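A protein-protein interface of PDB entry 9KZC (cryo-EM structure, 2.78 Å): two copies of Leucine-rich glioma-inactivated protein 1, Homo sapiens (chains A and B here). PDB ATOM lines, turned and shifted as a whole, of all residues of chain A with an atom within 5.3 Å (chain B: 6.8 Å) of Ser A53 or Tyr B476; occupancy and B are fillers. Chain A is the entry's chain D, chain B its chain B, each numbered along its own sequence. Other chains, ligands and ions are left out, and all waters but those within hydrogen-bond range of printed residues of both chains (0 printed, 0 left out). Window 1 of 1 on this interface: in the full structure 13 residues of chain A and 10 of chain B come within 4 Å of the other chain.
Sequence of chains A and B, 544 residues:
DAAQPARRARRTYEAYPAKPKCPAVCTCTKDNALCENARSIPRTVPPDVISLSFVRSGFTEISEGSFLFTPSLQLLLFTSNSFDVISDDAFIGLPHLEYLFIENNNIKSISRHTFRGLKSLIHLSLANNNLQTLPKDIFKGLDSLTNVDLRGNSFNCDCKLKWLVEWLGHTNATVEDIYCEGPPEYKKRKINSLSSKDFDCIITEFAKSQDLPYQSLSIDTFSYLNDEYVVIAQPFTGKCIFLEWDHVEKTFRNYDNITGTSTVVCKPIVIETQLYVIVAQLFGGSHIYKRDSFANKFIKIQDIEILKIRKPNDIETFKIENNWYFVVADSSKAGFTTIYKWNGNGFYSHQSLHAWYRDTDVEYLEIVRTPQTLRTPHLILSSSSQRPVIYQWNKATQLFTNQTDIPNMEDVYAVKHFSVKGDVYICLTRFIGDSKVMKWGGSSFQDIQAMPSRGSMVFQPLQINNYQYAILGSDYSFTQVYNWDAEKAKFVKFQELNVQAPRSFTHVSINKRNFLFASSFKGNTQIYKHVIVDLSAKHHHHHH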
ATOM      1  N   ASN A  32     -33.658 -18.676  32.606  1.00  0.00           N
ATOM      2  CA  ASN A  32     -32.578 -18.125  31.799  1.00  0.00           C
ATOM      3  C   ASN A  32     -32.789 -16.630  31.620  1.00  0.00           C
ATOM      4  O   ASN A  32     -33.894 -16.194  31.289  1.00  0.00           O
ATOM      5  CB  ASN A  32     -32.502 -18.818  30.434  1.00  0.00           C
ATOM      6  CG  ASN A  32     -31.354 -18.311  29.586  1.00  0.00           C
ATOM      7  OD1 ASN A  32     -30.184 -18.509  29.918  1.00  0.00           O
ATOM      8  ND2 ASN A  32     -31.681 -17.650  28.482  1.00  0.00           N
ATOM      9  N   ALA A  33     -31.731 -15.855  31.837  1.00  0.00           N
ATOM     10  CA  ALA A  33     -31.752 -14.414  31.635  1.00  0.00           C
ATOM     11  C   ALA A  33     -30.673 -14.036  30.634  1.00  0.00           C
ATOM     12  O   ALA A  33     -29.531 -14.494  30.745  1.00  0.00           O
ATOM     13  CB  ALA A  33     -31.540 -13.667  32.954  1.00  0.00           C
ATOM     14  N   LEU A  34     -31.034 -13.207  29.660  1.00  0.00           N
ATOM     15  CA  LEU A  34     -30.116 -12.755  28.616  1.00  0.00           C
ATOM     16  C   LEU A  34     -30.015 -11.236  28.724  1.00  0.00           C
ATOM     17  O   LEU A  34     -30.835 -10.503  28.166  1.00  0.00           O
ATOM     18  CB  LEU A  34     -30.593 -13.203  27.231  1.00  0.00           C
ATOM     19  CG  LEU A  34     -29.622 -13.048  26.057  1.00  0.00           C
ATOM     20  CD1 LEU A  34     -29.810 -14.187  25.072  1.00  0.00           C
ATOM     21  CD2 LEU A  34     -29.811 -11.711  25.355  1.00  0.00           C
ATOM     22  N   CYS A  35     -29.004 -10.767  29.450  1.00  0.00           N
ATOM     23  CA  CYS A  35     -28.793  -9.340  29.668  1.00  0.00           C
ATOM     24  C   CYS A  35     -27.944  -8.788  28.530  1.00  0.00           C
ATOM     25  O   CYS A  35     -26.763  -9.128  28.403  1.00  0.00           O
ATOM     26  CB  CYS A  35     -28.131  -9.098  31.021  1.00  0.00           C
ATOM     27  SG  CYS A  35     -29.139  -9.605  32.431  1.00  0.00           S
ATOM     28  N   SER A  51     -29.186 -19.933  34.644  1.00  0.00           N
ATOM     29  CA  SER A  51     -28.374 -19.619  33.472  1.00  0.00           C
ATOM     30  C   SER A  51     -28.444 -18.122  33.223  1.00  0.00           C
ATOM     31  O   SER A  51     -29.531 -17.586  32.980  1.00  0.00           O
ATOM     32  CB  SER A  51     -28.856 -20.396  32.249  1.00  0.00           C
ATOM     33  OG  SER A  51     -28.486 -21.760  32.336  1.00  0.00           O
ATOM     34  N   LEU A  52     -27.298 -17.450  33.280  1.00  0.00           N
ATOM     35  CA  LEU A  52     -27.214 -16.012  33.082  1.00  0.00           C
ATOM     36  C   LEU A  52     -26.214 -15.719  31.975  1.00  0.00           C
ATOM     37  O   LEU A  52     -25.158 -16.352  31.901  1.00  0.00           O
ATOM     38  CB  LEU A  52     -26.806 -15.300  34.377  1.00  0.00           C
ATOM     39  CG  LEU A  52     -26.725 -13.773  34.382  1.00  0.00           C
ATOM     40  CD1 LEU A  52     -28.071 -13.158  34.042  1.00  0.00           C
ATOM     41  CD2 LEU A  52     -26.241 -13.282  35.734  1.00  0.00           C
ATOM     42  N   SER A  53     -26.550 -14.759  31.116  1.00  0.00           N
ATOM     43  CA  SER A  53     -25.732 -14.428  29.960  1.00  0.00           C
ATOM     44  C   SER A  53     -25.548 -12.921  29.866  1.00  0.00           C
ATOM     45  O   SER A  53     -26.369 -12.146  30.362  1.00  0.00           O
ATOM     46  CB  SER A  53     -26.356 -14.958  28.661  1.00  0.00           C
ATOM     47  OG  SER A  53     -26.687 -16.330  28.777  1.00  0.00           O
ATOM     48  N   PHE A  54     -24.456 -12.515  29.220  1.00  0.00           N
ATOM     49  CA  PHE A  54     -24.132 -11.103  29.033  1.00  0.00           C
ATOM     50  C   PHE A  54     -23.582 -10.925  27.626  1.00  0.00           C
ATOM     51  O   PHE A  54     -22.469 -11.371  27.333  1.00  0.00           O
ATOM     52  CB  PHE A  54     -23.122 -10.623  30.076  1.00  0.00           C
ATOM     53  CG  PHE A  54     -23.667 -10.586  31.471  1.00  0.00           C
ATOM     54  CD1 PHE A  54     -24.361  -9.480  31.928  1.00  0.00           C
ATOM     55  CD2 PHE A  54     -23.489 -11.660  32.325  1.00  0.00           C
ATOM     56  CE1 PHE A  54     -24.864  -9.446  33.209  1.00  0.00           C
ATOM     57  CE2 PHE A  54     -23.990 -11.631  33.608  1.00  0.00           C
ATOM     58  CZ  PHE A  54     -24.679 -10.523  34.051  1.00  0.00           C
ATOM     59  N   VAL A  55     -24.353 -10.272  26.761  1.00  0.00           N
ATOM     60  CA  VAL A  55     -23.979 -10.067  25.367  1.00  0.00           C
ATOM     61  C   VAL A  55     -23.840  -8.572  25.117  1.00  0.00           C
ATOM     62  O   VAL A  55     -24.800  -7.816  25.304  1.00  0.00           O
ATOM     63  CB  VAL A  55     -25.009 -10.686  24.405  1.00  0.00           C
ATOM     64  CG1 VAL A  55     -24.597 -10.444  22.961  1.00  0.00           C
ATOM     65  CG2 VAL A  55     -25.169 -12.172  24.682  1.00  0.00           C
ATOM     66  N   LEU A  75     -25.033 -22.093  34.972  1.00  0.00           N
ATOM     67  CA  LEU A  75     -24.342 -21.741  33.742  1.00  0.00           C
ATOM     68  C   LEU A  75     -24.177 -20.231  33.693  1.00  0.00           C
ATOM     69  O   LEU A  75     -25.120 -19.488  33.974  1.00  0.00           O
ATOM     70  CB  LEU A  75     -25.114 -22.232  32.508  1.00  0.00           C
ATOM     71  CG  LEU A  75     -24.419 -22.120  31.148  1.00  0.00           C
ATOM     72  CD1 LEU A  75     -24.615 -23.396  30.350  1.00  0.00           C
ATOM     73  CD2 LEU A  75     -24.934 -20.917  30.374  1.00  0.00           C
ATOM     74  N   LEU A  76     -22.975 -19.781  33.343  1.00  0.00           N
ATOM     75  CA  LEU A  76     -22.682 -18.362  33.207  1.00  0.00           C
ATOM     76  C   LEU A  76     -21.976 -18.141  31.879  1.00  0.00           C
ATOM     77  O   LEU A  76     -21.044 -18.877  31.542  1.00  0.00           O
ATOM     78  CB  LEU A  76     -21.820 -17.857  34.368  1.00  0.00           C
ATOM     79  CG  LEU A  76     -21.697 -16.342  34.528  1.00  0.00           C
ATOM     80  CD1 LEU A  76     -23.047 -15.724  34.846  1.00  0.00           C
ATOM     81  CD2 LEU A  76     -20.693 -16.010  35.612  1.00  0.00           C
ATOM     82  N   LEU A  77     -22.419 -17.134  31.131  1.00  0.00           N
ATOM     83  CA  LEU A  77     -21.929 -16.917  29.779  1.00  0.00           C
ATOM     84  C   LEU A  77     -21.654 -15.439  29.555  1.00  0.00           C
ATOM     85  O   LEU A  77     -22.408 -14.580  30.018  1.00  0.00           O
ATOM     86  CB  LEU A  77     -22.940 -17.438  28.746  1.00  0.00           C
ATOM     87  CG  LEU A  77     -22.517 -17.553  27.281  1.00  0.00           C
ATOM     88  CD1 LEU A  77     -23.190 -18.753  26.647  1.00  0.00           C
ATOM     89  CD2 LEU A  77     -22.871 -16.293  26.515  1.00  0.00           C
ATOM     90  N   PHE B 431     -25.953 -30.372  22.231  1.00  0.00           N
ATOM     91  CA  PHE B 431     -26.515 -29.366  23.128  1.00  0.00           C
ATOM     92  C   PHE B 431     -25.429 -28.440  23.664  1.00  0.00           C
ATOM     93  O   PHE B 431     -25.436 -27.232  23.400  1.00  0.00           O
ATOM     94  CB  PHE B 431     -27.263 -30.042  24.276  1.00  0.00           C
ATOM     95  CG  PHE B 431     -28.066 -29.091  25.113  1.00  0.00           C
ATOM     96  CD1 PHE B 431     -29.154 -28.427  24.575  1.00  0.00           C
ATOM     97  CD2 PHE B 431     -27.731 -28.855  26.434  1.00  0.00           C
ATOM     98  CE1 PHE B 431     -29.894 -27.550  25.339  1.00  0.00           C
ATOM     99  CE2 PHE B 431     -28.467 -27.978  27.203  1.00  0.00           C
ATOM    100  CZ  PHE B 431     -29.549 -27.324  26.653  1.00  0.00           C
ATOM    101  N   ILE B 432     -24.486 -28.990  24.422  1.00  0.00           N
ATOM    102  CA  ILE B 432     -23.330 -28.256  24.919  1.00  0.00           C
ATOM    103  C   ILE B 432     -22.083 -28.919  24.360  1.00  0.00           C
ATOM    104  O   ILE B 432     -21.888 -30.128  24.531  1.00  0.00           O
ATOM    105  CB  ILE B 432     -23.287 -28.221  26.458  1.00  0.00           C
ATOM    106  CG1 ILE B 432     -24.528 -27.525  27.022  1.00  0.00           C
ATOM    107  CG2 ILE B 432     -22.016 -27.533  26.940  1.00  0.00           C
ATOM    108  CD1 ILE B 432     -24.419 -26.018  27.077  1.00  0.00           C
ATOM    109  N   ARG B 454     -24.037 -23.680  22.684  1.00  0.00           N
ATOM    110  CA  ARG B 454     -24.396 -23.312  24.054  1.00  0.00           C
ATOM    111  C   ARG B 454     -25.916 -23.400  24.149  1.00  0.00           C
ATOM    112  O   ARG B 454     -26.624 -22.452  23.805  1.00  0.00           O
ATOM    113  CB  ARG B 454     -23.873 -21.920  24.417  1.00  0.00           C
ATOM    114  CG  ARG B 454     -22.380 -21.884  24.709  1.00  0.00           C
ATOM    115  CD  ARG B 454     -21.564 -21.741  23.437  1.00  0.00           C
ATOM    116  NE  ARG B 454     -20.156 -21.481  23.707  1.00  0.00           N
ATOM    117  CZ  ARG B 454     -19.230 -22.426  23.787  1.00  0.00           C
ATOM    118  NH1 ARG B 454     -19.534 -23.705  23.645  1.00  0.00           N
ATOM    119  NH2 ARG B 454     -17.967 -22.081  24.016  1.00  0.00           N
ATOM    120  N   GLY B 455     -26.408 -24.539  24.624  1.00  0.00           N
ATOM    121  CA  GLY B 455     -27.838 -24.784  24.639  1.00  0.00           C
ATOM    122  C   GLY B 455     -28.438 -24.903  23.256  1.00  0.00           C
ATOM    123  O   GLY B 455     -29.517 -24.353  23.002  1.00  0.00           O
ATOM    124  N   SER B 456     -27.765 -25.612  22.354  1.00  0.00           N
ATOM    125  CA  SER B 456     -28.193 -25.717  20.966  1.00  0.00           C
ATOM    126  C   SER B 456     -29.072 -26.948  20.789  1.00  0.00           C
ATOM    127  O   SER B 456     -28.608 -28.079  20.963  1.00  0.00           O
ATOM    128  CB  SER B 456     -26.982 -25.785  20.039  1.00  0.00           C
ATOM    129  OG  SER B 456     -27.365 -26.207  18.743  1.00  0.00           O
ATOM    130  N   GLY B 473     -29.133 -22.780  16.649  1.00  0.00           N
ATOM    131  CA  GLY B 473     -29.855 -22.210  17.764  1.00  0.00           C
ATOM    132  C   GLY B 473     -29.063 -22.256  19.054  1.00  0.00           C
ATOM    133  O   GLY B 473     -28.038 -22.923  19.170  1.00  0.00           O
ATOM    134  N   SER B 474     -29.555 -21.517  20.046  1.00  0.00           N
ATOM    135  CA  SER B 474     -28.898 -21.467  21.346  1.00  0.00           C
ATOM    136  C   SER B 474     -29.912 -21.052  22.399  1.00  0.00           C
ATOM    137  O   SER B 474     -30.586 -20.030  22.242  1.00  0.00           O
ATOM    138  CB  SER B 474     -27.714 -20.494  21.328  1.00  0.00           C
ATOM    139  OG  SER B 474     -27.083 -20.441  22.594  1.00  0.00           O
ATOM    140  N   ASP B 475     -30.017 -21.846  23.464  1.00  0.00           N
ATOM    141  CA  ASP B 475     -30.904 -21.525  24.575  1.00  0.00           C
ATOM    142  C   ASP B 475     -30.287 -20.550  25.567  1.00  0.00           C
ATOM    143  O   ASP B 475     -31.016 -19.987  26.390  1.00  0.00           O
ATOM    144  CB  ASP B 475     -31.308 -22.803  25.313  1.00  0.00           C
ATOM    145  CG  ASP B 475     -32.356 -23.602  24.569  1.00  0.00           C
ATOM    146  OD1 ASP B 475     -32.494 -23.410  23.343  1.00  0.00           O
ATOM    147  OD2 ASP B 475     -33.043 -24.422  25.211  1.00  0.00           O
ATOM    148  N   TYR B 476     -28.972 -20.335  25.508  1.00  0.00           N
ATOM    149  CA  TYR B 476     -28.278 -19.494  26.469  1.00  0.00           C
ATOM    150  C   TYR B 476     -27.591 -18.286  25.851  1.00  0.00           C
ATOM    151  O   TYR B 476     -27.017 -17.482  26.592  1.00  0.00           O
ATOM    152  CB  TYR B 476     -27.232 -20.316  27.237  1.00  0.00           C
ATOM    153  CG  TYR B 476     -27.789 -21.560  27.885  1.00  0.00           C
ATOM    154  CD1 TYR B 476     -28.933 -21.506  28.666  1.00  0.00           C
ATOM    155  CD2 TYR B 476     -27.170 -22.789  27.716  1.00  0.00           C
ATOM    156  CE1 TYR B 476     -29.446 -22.640  29.260  1.00  0.00           C
ATOM    157  CE2 TYR B 476     -27.675 -23.929  28.306  1.00  0.00           C
ATOM    158  CZ  TYR B 476     -28.813 -23.848  29.076  1.00  0.00           C
ATOM    159  OH  TYR B 476     -29.321 -24.982  29.668  1.00  0.00           O
ATOM    160  N   SER B 477     -27.627 -18.134  24.532  1.00  0.00           N
ATOM    161  CA  SER B 477     -26.981 -17.012  23.867  1.00  0.00           C
ATOM    162  C   SER B 477     -27.770 -16.687  22.605  1.00  0.00           C
ATOM    163  O   SER B 477     -28.897 -17.154  22.419  1.00  0.00           O
ATOM    164  CB  SER B 477     -25.511 -17.336  23.568  1.00  0.00           C
ATOM    165  OG  SER B 477     -24.838 -16.211  23.035  1.00  0.00           O
ATOM    166  N   PHE B 478     -27.175 -15.878  21.735  1.00  0.00           N
ATOM    167  CA  PHE B 478     -27.813 -15.538  20.475  1.00  0.00           C
ATOM    168  C   PHE B 478     -27.817 -16.734  19.530  1.00  0.00           C
ATOM    169  O   PHE B 478     -27.042 -17.682  19.672  1.00  0.00           O
ATOM    170  CB  PHE B 478     -27.104 -14.358  19.810  1.00  0.00           C
ATOM    171  CG  PHE B 478     -27.695 -13.025  20.156  1.00  0.00           C
ATOM    172  CD1 PHE B 478     -27.965 -12.689  21.471  1.00  0.00           C
ATOM    173  CD2 PHE B 478     -27.987 -12.107  19.161  1.00  0.00           C
ATOM    174  CE1 PHE B 478     -28.511 -11.462  21.786  1.00  0.00           C
ATOM    175  CE2 PHE B 478     -28.534 -10.880  19.470  1.00  0.00           C
ATOM    176  CZ  PHE B 478     -28.796 -10.556  20.784  1.00  0.00           C
ATOM    177  N   ALA B 501     -35.044 -19.631  22.963  1.00  0.00           N
ATOM    178  CA  ALA B 501     -35.007 -21.089  22.920  1.00  0.00           C
ATOM    179  C   ALA B 501     -35.548 -21.620  21.597  1.00  0.00           C
ATOM    180  O   ALA B 501     -36.625 -22.226  21.569  1.00  0.00           O
ATOM    181  CB  ALA B 501     -35.799 -21.678  24.089  1.00  0.00           C
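ND2 of Asn A32 sits at hydrogen-bond distance from O of Asp B475, 3.2 Å away.
The backbone carbonyl oxygen (O) of Tyr B476 sits at hydrogen-bond distance from the side-chain hydroxyl (OG) of Ser A53 (2.5 Å).
The backbone carbonyl oxygen (O) of Arg B454 is in hydrogen-bond range of the backbone NH (N) of Asp B475 (3.5 Å).
The side-chain hydroxyl of Ser B474 is in hydrogen-bond range of the backbone NH of Ser B477 (3.1 Å).
The backbone NH (N) of Asp B475 sits at hydrogen-bond distance from the backbone carbonyl oxygen (O) of Gly B455 (2.6 Å).
The backbone NH (N) of Tyr B476 lies close to the side-chain hydroxyl (OG) of Ser B474 (3.5 Å).
The backbone NH of Ala A33 is in hydrogen-bond range of the backbone carbonyl oxygen of Ser A51 (3.0 Å).
The backbone NH (N) of Leu A52 sits at hydrogen-bond distance from the backbone carbonyl oxygen (O) of Leu A75, 3.1 Å away.
Asn A32 touches Tyr B476.
Leu A34 touches Phe B478.
Ser A51 touches Tyr B476.
Tyr B476 touches Leu A75.
CG of Arg B454 touches CD1 of Leu A77 (3.8 Å).
OG of Ser B477 touches CD2 of Leu A77 (3.998 Å).
Of the printed residues of chain B, Asn A32 touches Asp B475 and Tyr B476.
Of chain B, only Tyr B476 (2.5 Å) comes within 4 Å of Ser A53.
Printed residues of chain A within 4 Å of Asp B475: Asn A32 (3.2 Å).
Tyr B476 touches four residues of chain A.
The nearest residue of chain B that does not touch Ser A53 is Ser B477 (4.7 Å).
The nearest printed residue of chain B that does not touch Leu A77 is Tyr B476 (4.03 Å).
Of the 12 printed residues of chain A, 6 touch a printed residue of chain B.
Hydrophobic or aromatic side chains of chain A within 4 Å of the printed part of chain B: Leu A34, Leu A75 and Leu A77.
Along chain A the printed residues that touch a printed residue of chain B span positions 32 to 77.
Printed residues of chain B that touch a printed residue of chain A: Arg B454, Asp B475, Tyr B476, Ser B477 and Phe B478.
Among the printed residues, no Asp or Glu carboxylate lies within 4 Å of a Lys or Arg side-chain nitrogen of the other chain.
No position is printed for both chains.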
